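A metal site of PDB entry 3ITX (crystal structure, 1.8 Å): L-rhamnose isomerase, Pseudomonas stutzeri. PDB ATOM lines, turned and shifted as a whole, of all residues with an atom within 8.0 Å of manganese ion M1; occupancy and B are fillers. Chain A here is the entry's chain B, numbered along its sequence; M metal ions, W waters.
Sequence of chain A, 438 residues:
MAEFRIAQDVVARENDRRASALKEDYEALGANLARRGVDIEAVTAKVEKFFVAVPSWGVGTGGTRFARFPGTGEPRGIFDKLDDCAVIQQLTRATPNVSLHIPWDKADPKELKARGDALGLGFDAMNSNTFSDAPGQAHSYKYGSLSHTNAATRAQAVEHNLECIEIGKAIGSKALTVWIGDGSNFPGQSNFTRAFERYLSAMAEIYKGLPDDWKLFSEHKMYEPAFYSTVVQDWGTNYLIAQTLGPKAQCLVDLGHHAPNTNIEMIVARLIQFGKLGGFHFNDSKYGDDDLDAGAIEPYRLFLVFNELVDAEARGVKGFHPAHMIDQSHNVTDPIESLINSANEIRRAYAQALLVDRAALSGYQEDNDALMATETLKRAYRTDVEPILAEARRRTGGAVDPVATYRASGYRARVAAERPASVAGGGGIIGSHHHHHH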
ATOM      1  N   TRP A  57      -5.568  20.167  10.904  1.00  0.00           N
ATOM      2  CA  TRP A  57      -5.071  20.176   9.533  1.00  0.00           C
ATOM      3  C   TRP A  57      -4.270  18.935   9.160  1.00  0.00           C
ATOM      4  O   TRP A  57      -3.896  18.748   7.996  1.00  0.00           O
ATOM      5  CB  TRP A  57      -4.220  21.440   9.305  1.00  0.00           C
ATOM      6  CG  TRP A  57      -2.971  21.530  10.150  1.00  0.00           C
ATOM      7  CD1 TRP A  57      -1.713  21.156   9.791  1.00  0.00           C
ATOM      8  CD2 TRP A  57      -2.874  22.030  11.493  1.00  0.00           C
ATOM      9  NE1 TRP A  57      -0.832  21.389  10.826  1.00  0.00           N
ATOM     10  CE2 TRP A  57      -1.524  21.916  11.884  1.00  0.00           C
ATOM     11  CE3 TRP A  57      -3.809  22.555  12.405  1.00  0.00           C
ATOM     12  CZ2 TRP A  57      -1.069  22.322  13.150  1.00  0.00           C
ATOM     13  CZ3 TRP A  57      -3.356  22.947  13.668  1.00  0.00           C
ATOM     14  CH2 TRP A  57      -1.998  22.824  14.024  1.00  0.00           C
ATOM     15  N   ASN A 127      -4.096  27.877  17.189  1.00  0.00           N
ATOM     16  CA  ASN A 127      -2.956  28.196  16.334  1.00  0.00           C
ATOM     17  C   ASN A 127      -3.330  29.380  15.452  1.00  0.00           C
ATOM     18  O   ASN A 127      -4.310  29.311  14.703  1.00  0.00           O
ATOM     19  CB  ASN A 127      -2.595  26.999  15.456  1.00  0.00           C
ATOM     20  CG  ASN A 127      -1.975  25.862  16.243  1.00  0.00           C
ATOM     21  OD1 ASN A 127      -0.763  25.822  16.467  1.00  0.00           O
ATOM     22  ND2 ASN A 127      -2.804  24.917  16.672  1.00  0.00           N
ATOM     23  N   THR A 177      -0.702  29.079  20.349  1.00  0.00           N
ATOM     24  CA  THR A 177       0.592  28.732  19.786  1.00  0.00           C
ATOM     25  C   THR A 177       0.867  29.702  18.652  1.00  0.00           C
ATOM     26  O   THR A 177       0.049  29.861  17.735  1.00  0.00           O
ATOM     27  CB  THR A 177       0.609  27.294  19.226  1.00  0.00           C
ATOM     28  OG1 THR A 177       0.626  26.358  20.307  1.00  0.00           O
ATOM     29  CG2 THR A 177       1.846  27.068  18.350  1.00  0.00           C
ATOM     30  N   TRP A 179       3.424  30.505  15.636  1.00  0.00           N
ATOM     31  CA  TRP A 179       4.518  30.150  14.743  1.00  0.00           C
ATOM     32  C   TRP A 179       4.338  31.040  13.540  1.00  0.00           C
ATOM     33  O   TRP A 179       3.270  31.043  12.919  1.00  0.00           O
ATOM     34  CB  TRP A 179       4.462  28.696  14.250  1.00  0.00           C
ATOM     35  CG  TRP A 179       5.508  28.489  13.191  1.00  0.00           C
ATOM     36  CD1 TRP A 179       6.856  28.392  13.389  1.00  0.00           C
ATOM     37  CD2 TRP A 179       5.308  28.492  11.770  1.00  0.00           C
ATOM     38  NE1 TRP A 179       7.522  28.361  12.173  1.00  0.00           N
ATOM     39  CE2 TRP A 179       6.590  28.420  11.168  1.00  0.00           C
ATOM     40  CE3 TRP A 179       4.177  28.570  10.950  1.00  0.00           C
ATOM     41  CZ2 TRP A 179       6.772  28.417   9.778  1.00  0.00           C
ATOM     42  CZ3 TRP A 179       4.362  28.572   9.568  1.00  0.00           C
ATOM     43  CH2 TRP A 179       5.643  28.496   8.995  1.00  0.00           C
ATOM     44  N   GLU A 219       7.054  29.247  18.852  1.00  0.00           N
ATOM     45  CA  GLU A 219       7.716  28.105  18.242  1.00  0.00           C
ATOM     46  C   GLU A 219       8.860  28.513  17.320  1.00  0.00           C
ATOM     47  O   GLU A 219       8.651  29.227  16.349  1.00  0.00           O
ATOM     48  CB  GLU A 219       6.685  27.290  17.460  1.00  0.00           C
ATOM     49  CG  GLU A 219       7.219  26.046  16.781  1.00  0.00           C
ATOM     50  CD  GLU A 219       6.122  25.237  16.112  1.00  0.00           C
ATOM     51  OE1 GLU A 219       4.935  25.572  16.288  1.00  0.00           O
ATOM     52  OE2 GLU A 219       6.448  24.254  15.419  1.00  0.00           O
ATOM     53  N   HIS A 220      10.076  28.042  17.623  1.00  0.00           N
ATOM     54  CA  HIS A 220      11.229  28.375  16.803  1.00  0.00           C
ATOM     55  C   HIS A 220      11.371  27.438  15.604  1.00  0.00           C
ATOM     56  O   HIS A 220      10.892  26.309  15.620  1.00  0.00           O
ATOM     57  CB  HIS A 220      12.516  28.339  17.633  1.00  0.00           C
ATOM     58  CG  HIS A 220      12.831  27.005  18.232  1.00  0.00           C
ATOM     59  ND1 HIS A 220      12.415  26.633  19.495  1.00  0.00           N
ATOM     60  CD2 HIS A 220      13.530  25.948  17.740  1.00  0.00           C
ATOM     61  CE1 HIS A 220      12.844  25.408  19.758  1.00  0.00           C
ATOM     62  NE2 HIS A 220      13.524  24.968  18.707  1.00  0.00           N
ATOM     63  N   LYS A 221      12.048  27.933  14.574  1.00  0.00           N
ATOM     64  CA  LYS A 221      12.280  27.153  13.353  1.00  0.00           C
ATOM     65  C   LYS A 221      13.485  27.764  12.648  1.00  0.00           C
ATOM     66  O   LYS A 221      13.531  28.972  12.412  1.00  0.00           O
ATOM     67  CB  LYS A 221      11.055  27.221  12.448  1.00  0.00           C
ATOM     68  CG  LYS A 221      11.119  26.254  11.276  1.00  0.00           C
ATOM     69  CD  LYS A 221       9.866  26.281  10.425  1.00  0.00           C
ATOM     70  CE  LYS A 221       9.978  25.298   9.272  1.00  0.00           C
ATOM     71  NZ  LYS A 221       8.764  25.322   8.408  1.00  0.00           N
ATOM     72  N   LEU A 252       7.928  26.141  22.513  1.00  0.00           N
ATOM     73  CA  LEU A 252       7.512  24.894  21.886  1.00  0.00           C
ATOM     74  C   LEU A 252       8.667  24.339  21.062  1.00  0.00           C
ATOM     75  O   LEU A 252       9.257  25.051  20.248  1.00  0.00           O
ATOM     76  CB  LEU A 252       6.325  25.126  20.963  1.00  0.00           C
ATOM     77  CG  LEU A 252       4.942  25.272  21.591  1.00  0.00           C
ATOM     78  CD1 LEU A 252       3.925  25.565  20.502  1.00  0.00           C
ATOM     79  CD2 LEU A 252       4.576  23.987  22.328  1.00  0.00           C
ATOM     80  N   VAL A 253       8.996  23.075  21.290  1.00  0.00           N
ATOM     81  CA  VAL A 253      10.080  22.407  20.566  1.00  0.00           C
ATOM     82  C   VAL A 253       9.491  21.464  19.526  1.00  0.00           C
ATOM     83  O   VAL A 253       8.853  20.471  19.874  1.00  0.00           O
ATOM     84  CB  VAL A 253      10.966  21.582  21.523  1.00  0.00           C
ATOM     85  CG1 VAL A 253      12.111  20.941  20.754  1.00  0.00           C
ATOM     86  CG2 VAL A 253      11.505  22.475  22.645  1.00  0.00           C
ATOM     87  N   ASP A 254       9.695  21.780  18.246  1.00  0.00           N
ATOM     88  CA  ASP A 254       9.203  20.940  17.157  1.00  0.00           C
ATOM     89  C   ASP A 254      10.417  20.191  16.608  1.00  0.00           C
ATOM     90  O   ASP A 254      11.338  20.794  16.064  1.00  0.00           O
ATOM     91  CB  ASP A 254       8.562  21.810  16.066  1.00  0.00           C
ATOM     92  CG  ASP A 254       7.912  20.984  14.979  1.00  0.00           C
ATOM     93  OD1 ASP A 254       8.580  20.081  14.452  1.00  0.00           O
ATOM     94  OD2 ASP A 254       6.742  21.246  14.641  1.00  0.00           O
ATOM     95  N   LEU A 255      10.399  18.876  16.767  1.00  0.00           N
ATOM     96  CA  LEU A 255      11.521  18.021  16.372  1.00  0.00           C
ATOM     97  C   LEU A 255      12.252  18.347  15.078  1.00  0.00           C
ATOM     98  O   LEU A 255      13.475  18.478  15.082  1.00  0.00           O
ATOM     99  CB  LEU A 255      11.070  16.552  16.365  1.00  0.00           C
ATOM    100  CG  LEU A 255      12.173  15.490  16.390  1.00  0.00           C
ATOM    101  CD1 LEU A 255      11.621  14.198  16.960  1.00  0.00           C
ATOM    102  CD2 LEU A 255      12.741  15.276  14.996  1.00  0.00           C
ATOM    103  N   GLY A 256      11.517  18.495  13.979  1.00  0.00           N
ATOM    104  CA  GLY A 256      12.168  18.778  12.710  1.00  0.00           C
ATOM    105  C   GLY A 256      12.576  20.212  12.422  1.00  0.00           C
ATOM    106  O   GLY A 256      12.916  20.537  11.288  1.00  0.00           O
ATOM    107  N   HIS A 257      12.566  21.072  13.440  1.00  0.00           N
ATOM    108  CA  HIS A 257      12.906  22.480  13.238  1.00  0.00           C
ATOM    109  C   HIS A 257      14.318  22.881  13.658  1.00  0.00           C
ATOM    110  O   HIS A 257      14.583  24.069  13.869  1.00  0.00           O
ATOM    111  CB  HIS A 257      11.923  23.377  13.989  1.00  0.00           C
ATOM    112  CG  HIS A 257      10.531  23.316  13.456  1.00  0.00           C
ATOM    113  ND1 HIS A 257       9.561  24.220  13.817  1.00  0.00           N
ATOM    114  CD2 HIS A 257       9.937  22.446  12.599  1.00  0.00           C
ATOM    115  CE1 HIS A 257       8.430  23.927  13.203  1.00  0.00           C
ATOM    116  NE2 HIS A 257       8.636  22.845  12.462  1.00  0.00           N
ATOM    117  N   PHE A 280       6.090  19.847  23.260  1.00  0.00           N
ATOM    118  CA  PHE A 280       6.889  19.286  22.182  1.00  0.00           C
ATOM    119  C   PHE A 280       5.974  18.957  21.010  1.00  0.00           C
ATOM    120  O   PHE A 280       4.899  18.394  21.196  1.00  0.00           O
ATOM    121  CB  PHE A 280       7.596  18.002  22.675  1.00  0.00           C
ATOM    122  CG  PHE A 280       8.748  17.569  21.816  1.00  0.00           C
ATOM    123  CD1 PHE A 280      10.036  18.053  22.044  1.00  0.00           C
ATOM    124  CD2 PHE A 280       8.550  16.685  20.756  1.00  0.00           C
ATOM    125  CE1 PHE A 280      11.114  17.657  21.240  1.00  0.00           C
ATOM    126  CE2 PHE A 280       9.616  16.285  19.947  1.00  0.00           C
ATOM    127  CZ  PHE A 280      10.897  16.775  20.186  1.00  0.00           C
ATOM    128  N   HIS A 281       6.398  19.319  19.803  1.00  0.00           N
ATOM    129  CA  HIS A 281       5.622  19.004  18.602  1.00  0.00           C
ATOM    130  C   HIS A 281       6.329  17.826  17.947  1.00  0.00           C
ATOM    131  O   HIS A 281       7.483  17.933  17.515  1.00  0.00           O
ATOM    132  CB  HIS A 281       5.562  20.194  17.640  1.00  0.00           C
ATOM    133  CG  HIS A 281       4.471  21.170  17.973  1.00  0.00           C
ATOM    134  ND1 HIS A 281       4.110  22.202  17.132  1.00  0.00           N
ATOM    135  CD2 HIS A 281       3.643  21.252  19.048  1.00  0.00           C
ATOM    136  CE1 HIS A 281       3.120  22.880  17.667  1.00  0.00           C
ATOM    137  NE2 HIS A 281       2.815  22.328  18.835  1.00  0.00           N
ATOM    138  N   PHE A 282       5.626  16.702  17.896  1.00  0.00           N
ATOM    139  CA  PHE A 282       6.156  15.465  17.357  1.00  0.00           C
ATOM    140  C   PHE A 282       6.019  15.269  15.860  1.00  0.00           C
ATOM    141  O   PHE A 282       5.013  15.624  15.243  1.00  0.00           O
ATOM    142  CB  PHE A 282       5.507  14.285  18.081  1.00  0.00           C
ATOM    143  CG  PHE A 282       5.819  14.252  19.556  1.00  0.00           C
ATOM    144  CD1 PHE A 282       7.022  13.736  20.014  1.00  0.00           C
ATOM    145  CD2 PHE A 282       4.908  14.743  20.483  1.00  0.00           C
ATOM    146  CE1 PHE A 282       7.329  13.713  21.379  1.00  0.00           C
ATOM    147  CE2 PHE A 282       5.193  14.738  21.843  1.00  0.00           C
ATOM    148  CZ  PHE A 282       6.403  14.216  22.291  1.00  0.00           C
ATOM    149  N   ASN A 283       7.067  14.683  15.286  1.00  0.00           N
ATOM    150  CA  ASN A 283       7.194  14.344  13.877  1.00  0.00           C
ATOM    151  C   ASN A 283       8.600  13.800  13.738  1.00  0.00           C
ATOM    152  O   ASN A 283       9.355  13.770  14.717  1.00  0.00           O
ATOM    153  CB  ASN A 283       6.999  15.579  12.976  1.00  0.00           C
ATOM    154  CG  ASN A 283       7.778  16.799  13.462  1.00  0.00           C
ATOM    155  OD1 ASN A 283       7.188  17.819  13.819  1.00  0.00           O
ATOM    156  ND2 ASN A 283       9.107  16.707  13.455  1.00  0.00           N
ATOM    157  N   ASP A 289      12.673  20.137   7.623  1.00  0.00           N
ATOM    158  CA  ASP A 289      11.433  20.042   8.383  1.00  0.00           C
ATOM    159  C   ASP A 289      10.496  19.145   7.582  1.00  0.00           C
ATOM    160  O   ASP A 289       9.457  19.570   7.097  1.00  0.00           O
ATOM    161  CB  ASP A 289      10.824  21.430   8.569  1.00  0.00           C
ATOM    162  CG  ASP A 289       9.540  21.392   9.371  1.00  0.00           C
ATOM    163  OD1 ASP A 289       9.440  20.525  10.254  1.00  0.00           O
ATOM    164  OD2 ASP A 289       8.644  22.232   9.110  1.00  0.00           O
ATOM    165  N   ASP A 291       8.449  16.818   8.399  1.00  0.00           N
ATOM    166  CA  ASP A 291       7.112  16.566   8.947  1.00  0.00           C
ATOM    167  C   ASP A 291       6.606  15.141   8.709  1.00  0.00           C
ATOM    168  O   ASP A 291       5.423  14.943   8.412  1.00  0.00           O
ATOM    169  CB  ASP A 291       6.103  17.567   8.355  1.00  0.00           C
ATOM    170  CG  ASP A 291       6.337  18.989   8.850  1.00  0.00           C
ATOM    171  OD1 ASP A 291       6.750  19.133  10.024  1.00  0.00           O
ATOM    172  OD2 ASP A 291       6.105  19.947   8.088  1.00  0.00           O
ATOM    173  N   MET A 325       1.770  17.875  21.030  1.00  0.00           N
ATOM    174  CA  MET A 325       0.943  17.811  19.836  1.00  0.00           C
ATOM    175  C   MET A 325       1.711  17.160  18.720  1.00  0.00           C
ATOM    176  O   MET A 325       2.940  17.226  18.664  1.00  0.00           O
ATOM    177  CB  MET A 325       0.517  19.217  19.388  1.00  0.00           C
ATOM    178  CG  MET A 325      -0.377  19.206  18.144  1.00  0.00           C
ATOM    179  SD  MET A 325      -0.796  20.828  17.456  1.00  0.00           S
ATOM    180  CE  MET A 325       0.543  21.044  16.255  1.00  0.00           C
ATOM    181  N   ILE A 326       0.981  16.496  17.821  1.00  0.00           N
ATOM    182  CA  ILE A 326       1.598  15.886  16.658  1.00  0.00           C
ATOM    183  C   ILE A 326       1.494  16.968  15.597  1.00  0.00           C
ATOM    184  O   ILE A 326       0.445  17.582  15.433  1.00  0.00           O
ATOM    185  CB  ILE A 326       0.800  14.645  16.182  1.00  0.00           C
ATOM    186  CG1 ILE A 326       0.829  13.570  17.269  1.00  0.00           C
ATOM    187  CG2 ILE A 326       1.397  14.102  14.887  1.00  0.00           C
ATOM    188  CD1 ILE A 326      -0.024  12.343  16.936  1.00  0.00           C
ATOM    189  N   ASP A 327       2.590  17.253  14.900  1.00  0.00           N
ATOM    190  CA  ASP A 327       2.587  18.273  13.869  1.00  0.00           C
ATOM    191  C   ASP A 327       3.278  17.666  12.674  1.00  0.00           C
ATOM    192  O   ASP A 327       4.500  17.769  12.529  1.00  0.00           O
ATOM    193  CB  ASP A 327       3.332  19.528  14.343  1.00  0.00           C
ATOM    194  CG  ASP A 327       3.202  20.679  13.373  1.00  0.00           C
ATOM    195  OD1 ASP A 327       2.434  20.560  12.391  1.00  0.00           O
ATOM    196  OD2 ASP A 327       3.869  21.711  13.584  1.00  0.00           O
ATOM    197  N   GLN A 328       2.493  17.016  11.827  1.00  0.00           N
ATOM    198  CA  GLN A 328       3.029  16.322  10.666  1.00  0.00           C
ATOM    199  C   GLN A 328       2.277  16.638   9.387  1.00  0.00           C
ATOM    200  O   GLN A 328       1.209  17.254   9.412  1.00  0.00           O
ATOM    201  CB  GLN A 328       2.988  14.815  10.923  1.00  0.00           C
ATOM    202  CG  GLN A 328       3.772  14.386  12.169  1.00  0.00           C
ATOM    203  CD  GLN A 328       3.486  12.951  12.591  1.00  0.00           C
ATOM    204  OE1 GLN A 328       4.113  12.446  13.525  1.00  0.00           O
ATOM    205  NE2 GLN A 328       2.548  12.294  11.915  1.00  0.00           N
HETATM  206 MN    MN M   1       5.161  22.646  15.086  1.00  0.00          MN
HETATM  207 MN    MN M   2       7.644  21.072  10.798  1.00  0.00          MN
HETATM  208  O   HOH W   1       5.404  23.574  12.808  1.00  0.00           O
HETATM  209  O   HOH W   2       3.567  24.746  14.059  1.00  0.00           O
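N of Asp 327 is in hydrogen-bond range of O of Phe 282 (2.9 Å).
The side-chain amide oxygen (OD1) of Asn 283 lies close to the backbone carbonyl oxygen (O) of Asp 327, 3.0 Å away.
O of His 281 sits at hydrogen-bond distance from N of Leu 255 (3.2 Å).
The side-chain carboxylate of Asp 254 sits close to a ring nitrogen (NE2) of His 257 (3.4 Å).
The backbone carbonyl oxygen of His 220 lies within hydrogen-bond range of a ring nitrogen (ND1) of His 257, at 3.1 Å.
The side-chain amide oxygen of Asn 283 lies close to the side-chain carboxylate of Asp 254 (2.7 Å).
OD1 of Asp 254 sits close to N of Gly 256 (3.4 Å).
O of Val 253 is in hydrogen-bond range of N of His 281, at 2.7 Å.
Residues that only touch manganese ion M1: His 257.
Within 4 Å of manganese ion M1: Glu 219, Asp 254, His 257, His 281 and Asp 327.
The nearest printed residue that does not touch manganese ion M1 is Met 325 (5.0 Å).
OE2 of Glu 219 binds manganese ion M1, at 2.1 Å.
Manganese ion M1 is bound by OD2 of Asp 254 (2.2 Å).
Manganese ion M1 is bound by OD2 of Asp 327 (2.2 Å).
A ring nitrogen (ND1) of His 281 binds manganese ion M1.
Manganese ion M1 is bound by water W1.
Manganese ion M1 has five donor atoms within binding distance.
Slightly farther from manganese ion M1 lies water W2 (2.8 Å).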
